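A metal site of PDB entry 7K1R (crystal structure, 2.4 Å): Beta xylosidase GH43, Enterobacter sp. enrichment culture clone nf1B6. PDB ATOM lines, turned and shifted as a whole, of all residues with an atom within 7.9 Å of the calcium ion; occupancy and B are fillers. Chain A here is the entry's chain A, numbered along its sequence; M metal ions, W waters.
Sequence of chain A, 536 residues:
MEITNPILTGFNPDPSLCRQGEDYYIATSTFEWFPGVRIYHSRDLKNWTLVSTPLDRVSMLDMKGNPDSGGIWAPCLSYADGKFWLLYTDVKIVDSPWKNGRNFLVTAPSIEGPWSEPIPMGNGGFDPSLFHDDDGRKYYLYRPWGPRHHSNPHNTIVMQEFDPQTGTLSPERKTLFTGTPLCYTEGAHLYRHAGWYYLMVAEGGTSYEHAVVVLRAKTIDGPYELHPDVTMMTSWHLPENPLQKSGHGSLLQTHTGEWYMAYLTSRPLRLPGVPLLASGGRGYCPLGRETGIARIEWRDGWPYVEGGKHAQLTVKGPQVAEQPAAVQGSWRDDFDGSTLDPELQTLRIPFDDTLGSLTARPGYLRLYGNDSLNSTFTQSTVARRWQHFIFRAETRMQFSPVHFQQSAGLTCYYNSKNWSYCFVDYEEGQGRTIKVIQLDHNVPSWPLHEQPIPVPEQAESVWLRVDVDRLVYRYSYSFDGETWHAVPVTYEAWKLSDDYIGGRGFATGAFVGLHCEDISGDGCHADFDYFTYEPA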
ATOM      1  N   ARG A 332      25.193   7.210  19.594  1.00  0.00           N
ATOM      2  CA  ARG A 332      25.298   6.757  20.975  1.00  0.00           C
ATOM      3  C   ARG A 332      26.688   6.202  21.226  1.00  0.00           C
ATOM      4  O   ARG A 332      27.304   5.589  20.344  1.00  0.00           O
ATOM      5  CB  ARG A 332      24.232   5.699  21.305  1.00  0.00           C
ATOM      6  CG  ARG A 332      24.477   4.319  20.723  1.00  0.00           C
ATOM      7  CD  ARG A 332      23.365   3.350  21.114  1.00  0.00           C
ATOM      8  NE  ARG A 332      23.351   3.086  22.553  1.00  0.00           N
ATOM      9  CZ  ARG A 332      22.270   3.203  23.314  1.00  0.00           C
ATOM     10  NH1 ARG A 332      21.116   3.589  22.796  1.00  0.00           N
ATOM     11  NH2 ARG A 332      22.354   2.940  24.621  1.00  0.00           N
ATOM     12  N   ASP A 333      27.184   6.442  22.444  1.00  0.00           N
ATOM     13  CA  ASP A 333      28.415   5.844  22.940  1.00  0.00           C
ATOM     14  C   ASP A 333      28.046   4.971  24.124  1.00  0.00           C
ATOM     15  O   ASP A 333      27.544   5.467  25.138  1.00  0.00           O
ATOM     16  CB  ASP A 333      29.424   6.914  23.343  1.00  0.00           C
ATOM     17  CG  ASP A 333      30.832   6.356  23.537  1.00  0.00           C
ATOM     18  OD1 ASP A 333      30.975   5.130  23.698  1.00  0.00           O
ATOM     19  OD2 ASP A 333      31.785   7.151  23.534  1.00  0.00           O
ATOM     20  N   ASP A 334      28.281   3.665  24.003  1.00  0.00           N
ATOM     21  CA  ASP A 334      28.045   2.727  25.090  1.00  0.00           C
ATOM     22  C   ASP A 334      29.263   2.541  25.969  1.00  0.00           C
ATOM     23  O   ASP A 334      29.219   1.752  26.920  1.00  0.00           O
ATOM     24  CB  ASP A 334      27.589   1.376  24.533  1.00  0.00           C
ATOM     25  CG  ASP A 334      26.181   1.421  23.977  1.00  0.00           C
ATOM     26  OD1 ASP A 334      25.217   1.514  24.768  1.00  0.00           O
ATOM     27  OD2 ASP A 334      26.032   1.376  22.731  1.00  0.00           O
ATOM     28  N   PHE A 335      30.369   3.235  25.667  1.00  0.00           N
ATOM     29  CA  PHE A 335      31.554   3.257  26.522  1.00  0.00           C
ATOM     30  C   PHE A 335      32.113   1.851  26.739  1.00  0.00           C
ATOM     31  O   PHE A 335      32.572   1.499  27.825  1.00  0.00           O
ATOM     32  CB  PHE A 335      31.260   3.940  27.851  1.00  0.00           C
ATOM     33  CG  PHE A 335      30.738   5.347  27.705  1.00  0.00           C
ATOM     34  CD1 PHE A 335      31.429   6.278  26.934  1.00  0.00           C
ATOM     35  CD2 PHE A 335      29.571   5.738  28.324  1.00  0.00           C
ATOM     36  CE1 PHE A 335      30.944   7.571  26.798  1.00  0.00           C
ATOM     37  CE2 PHE A 335      29.086   7.031  28.188  1.00  0.00           C
ATOM     38  CZ  PHE A 335      29.773   7.947  27.425  1.00  0.00           C
ATOM     39  N   ASP A 336      32.081   1.041  25.673  1.00  0.00           N
ATOM     40  CA  ASP A 336      32.540  -0.338  25.736  1.00  0.00           C
ATOM     41  C   ASP A 336      34.000  -0.509  25.352  1.00  0.00           C
ATOM     42  O   ASP A 336      34.590  -1.560  25.660  1.00  0.00           O
ATOM     43  CB  ASP A 336      31.681  -1.227  24.830  1.00  0.00           C
ATOM     44  CG  ASP A 336      30.316  -1.510  25.404  1.00  0.00           C
ATOM     45  OD1 ASP A 336      30.233  -1.842  26.610  1.00  0.00           O
ATOM     46  OD2 ASP A 336      29.319  -1.387  24.665  1.00  0.00           O
ATOM     47  N   ARG A 361      35.939   1.046  35.384  1.00  0.00           N
ATOM     48  CA  ARG A 361      34.719   0.234  35.374  1.00  0.00           C
ATOM     49  C   ARG A 361      34.342  -0.006  33.925  1.00  0.00           C
ATOM     50  O   ARG A 361      33.661   0.821  33.297  1.00  0.00           O
ATOM     51  CB  ARG A 361      33.586   0.920  36.138  1.00  0.00           C
ATOM     52  CG  ARG A 361      32.299   0.120  36.175  1.00  0.00           C
ATOM     53  CD  ARG A 361      31.345   0.647  37.230  1.00  0.00           C
ATOM     54  NE  ARG A 361      30.175  -0.219  37.382  1.00  0.00           N
ATOM     55  CZ  ARG A 361      28.964   0.223  37.688  1.00  0.00           C
ATOM     56  NH1 ARG A 361      28.756   1.524  37.886  1.00  0.00           N
ATOM     57  NH2 ARG A 361      27.959  -0.629  37.817  1.00  0.00           N
ATOM     58  N   PRO A 362      34.782  -1.120  33.349  1.00  0.00           N
ATOM     59  CA  PRO A 362      34.510  -1.370  31.924  1.00  0.00           C
ATOM     60  C   PRO A 362      33.018  -1.406  31.632  1.00  0.00           C
ATOM     61  O   PRO A 362      32.216  -1.905  32.436  1.00  0.00           O
ATOM     62  CB  PRO A 362      35.156  -2.744  31.677  1.00  0.00           C
ATOM     63  CG  PRO A 362      36.191  -2.871  32.763  1.00  0.00           C
ATOM     64  CD  PRO A 362      35.594  -2.181  33.955  1.00  0.00           C
ATOM     65  N   GLY A 363      32.653  -0.859  30.480  1.00  0.00           N
ATOM     66  CA  GLY A 363      31.260  -0.694  30.126  1.00  0.00           C
ATOM     67  C   GLY A 363      30.637   0.600  30.609  1.00  0.00           C
ATOM     68  O   GLY A 363      29.504   0.912  30.227  1.00  0.00           O
ATOM     69  N   TYR A 364      31.342   1.360  31.449  1.00  0.00           N
ATOM     70  CA  TYR A 364      30.867   2.644  31.931  1.00  0.00           C
ATOM     71  C   TYR A 364      31.925   3.710  31.687  1.00  0.00           C
ATOM     72  O   TYR A 364      33.121   3.420  31.637  1.00  0.00           O
ATOM     73  CB  TYR A 364      30.561   2.613  33.440  1.00  0.00           C
ATOM     74  CG  TYR A 364      29.360   1.773  33.833  1.00  0.00           C
ATOM     75  CD1 TYR A 364      29.412   0.392  33.801  1.00  0.00           C
ATOM     76  CD2 TYR A 364      28.184   2.377  34.253  1.00  0.00           C
ATOM     77  CE1 TYR A 364      28.324  -0.377  34.161  1.00  0.00           C
ATOM     78  CE2 TYR A 364      27.078   1.622  34.617  1.00  0.00           C
ATOM     79  CZ  TYR A 364      27.158   0.249  34.576  1.00  0.00           C
ATOM     80  OH  TYR A 364      26.075  -0.513  34.940  1.00  0.00           O
ATOM     81  N   LEU A 365      31.462   4.941  31.513  1.00  0.00           N
ATOM     82  CA  LEU A 365      32.347   6.104  31.525  1.00  0.00           C
ATOM     83  C   LEU A 365      32.342   6.671  32.944  1.00  0.00           C
ATOM     84  O   LEU A 365      31.320   7.191  33.406  1.00  0.00           O
ATOM     85  CB  LEU A 365      31.904   7.160  30.513  1.00  0.00           C
ATOM     86  CG  LEU A 365      32.581   8.513  30.697  1.00  0.00           C
ATOM     87  CD1 LEU A 365      34.069   8.438  30.364  1.00  0.00           C
ATOM     88  CD2 LEU A 365      31.908   9.595  29.869  1.00  0.00           C
ATOM     89  N   ARG A 396      22.246   7.030  31.485  1.00  0.00           N
ATOM     90  CA  ARG A 396      21.965   6.322  32.730  1.00  0.00           C
ATOM     91  C   ARG A 396      23.178   6.482  33.640  1.00  0.00           C
ATOM     92  O   ARG A 396      24.290   6.118  33.251  1.00  0.00           O
ATOM     93  CB  ARG A 396      21.658   4.848  32.486  1.00  0.00           C
ATOM     94  CG  ARG A 396      21.660   4.013  33.763  1.00  0.00           C
ATOM     95  CD  ARG A 396      21.109   2.619  33.535  1.00  0.00           C
ATOM     96  NE  ARG A 396      22.154   1.676  33.133  1.00  0.00           N
ATOM     97  CZ  ARG A 396      22.965   1.045  33.975  1.00  0.00           C
ATOM     98  NH1 ARG A 396      22.861   1.259  35.283  1.00  0.00           N
ATOM     99  NH2 ARG A 396      23.869   0.207  33.517  1.00  0.00           N
ATOM    100  N   PHE A 528      28.674   6.489  34.046  1.00  0.00           N
ATOM    101  CA  PHE A 528      27.671   6.683  33.000  1.00  0.00           C
ATOM    102  C   PHE A 528      27.675   5.464  32.089  1.00  0.00           C
ATOM    103  O   PHE A 528      28.677   5.177  31.435  1.00  0.00           O
ATOM    104  CB  PHE A 528      27.954   7.956  32.188  1.00  0.00           C
ATOM    105  CG  PHE A 528      27.878   9.218  33.004  1.00  0.00           C
ATOM    106  CD1 PHE A 528      26.689   9.915  33.116  1.00  0.00           C
ATOM    107  CD2 PHE A 528      29.005   9.709  33.654  1.00  0.00           C
ATOM    108  CE1 PHE A 528      26.617  11.075  33.861  1.00  0.00           C
ATOM    109  CE2 PHE A 528      28.937  10.870  34.391  1.00  0.00           C
ATOM    110  CZ  PHE A 528      27.741  11.560  34.499  1.00  0.00           C
ATOM    111  N   ASP A 529      26.543   4.760  32.049  1.00  0.00           N
ATOM    112  CA  ASP A 529      26.462   3.572  31.211  1.00  0.00           C
ATOM    113  C   ASP A 529      26.538   3.931  29.729  1.00  0.00           C
ATOM    114  O   ASP A 529      27.295   3.329  28.966  1.00  0.00           O
ATOM    115  CB  ASP A 529      25.174   2.804  31.514  1.00  0.00           C
ATOM    116  CG  ASP A 529      25.153   1.432  30.867  1.00  0.00           C
ATOM    117  OD1 ASP A 529      26.131   0.683  31.030  1.00  0.00           O
ATOM    118  OD2 ASP A 529      24.141   1.103  30.202  1.00  0.00           O
ATOM    119  N   TYR A 530      25.774   4.943  29.306  1.00  0.00           N
ATOM    120  CA  TYR A 530      25.730   5.305  27.902  1.00  0.00           C
ATOM    121  C   TYR A 530      25.396   6.780  27.759  1.00  0.00           C
ATOM    122  O   TYR A 530      25.006   7.449  28.713  1.00  0.00           O
ATOM    123  CB  TYR A 530      24.719   4.438  27.127  1.00  0.00           C
ATOM    124  CG  TYR A 530      23.297   4.549  27.646  1.00  0.00           C
ATOM    125  CD1 TYR A 530      22.479   5.615  27.278  1.00  0.00           C
ATOM    126  CD2 TYR A 530      22.771   3.576  28.477  1.00  0.00           C
ATOM    127  CE1 TYR A 530      21.185   5.721  27.734  1.00  0.00           C
ATOM    128  CE2 TYR A 530      21.460   3.669  28.936  1.00  0.00           C
ATOM    129  CZ  TYR A 530      20.682   4.741  28.565  1.00  0.00           C
ATOM    130  OH  TYR A 530      19.385   4.833  29.029  1.00  0.00           O
ATOM    131  N   PHE A 531      25.558   7.268  26.533  1.00  0.00           N
ATOM    132  CA  PHE A 531      25.178   8.626  26.152  1.00  0.00           C
ATOM    133  C   PHE A 531      24.561   8.555  24.769  1.00  0.00           C
ATOM    134  O   PHE A 531      25.186   8.031  23.842  1.00  0.00           O
ATOM    135  CB  PHE A 531      26.391   9.566  26.155  1.00  0.00           C
ATOM    136  CG  PHE A 531      26.036  11.025  26.143  1.00  0.00           C
ATOM    137  CD1 PHE A 531      24.791  11.452  26.576  1.00  0.00           C
ATOM    138  CD2 PHE A 531      26.944  11.965  25.702  1.00  0.00           C
ATOM    139  CE1 PHE A 531      24.454  12.790  26.564  1.00  0.00           C
ATOM    140  CE2 PHE A 531      26.625  13.318  25.688  1.00  0.00           C
ATOM    141  CZ  PHE A 531      25.379  13.730  26.119  1.00  0.00           C
HETATM  142 CA    CA M   1      27.622   0.991  28.777  1.00  0.00          CA
HETATM  143  O   HOH W   1      27.840  -1.483  28.332  1.00  0.00           O
HETATM  144  O   HOH W   2      25.596   0.030  27.229  1.00  0.00           O
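NH2 of Arg 396 lies within salt-bridge range of OD2 of Asp 529, 3.4 Å away.
NE of Arg 332 is in salt-bridge range of OD2 of Asp 334 (3.2 Å).
Within 4 Å of the calcium ion: Asp 334, Gly 363 and Asp 529.
The nearest printed residue that does not touch the calcium ion is Tyr 530 (4.4 Å).
The calcium ion is bound by the backbone carbonyl oxygen (O) of Asp 529, the backbone carbonyl oxygen (O) of Gly 363, water W1, the backbone carbonyl oxygen (O) of Asp 334, the side-chain carboxylate (OD1) of Asp 529 and water W2.
The calcium ion has six donor atoms within binding distance.
Water W2 lies within hydrogen-bond range of the side-chain carboxylate (OD1) of Asp 334 and the side-chain carboxylate (OD2) of Asp 529.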
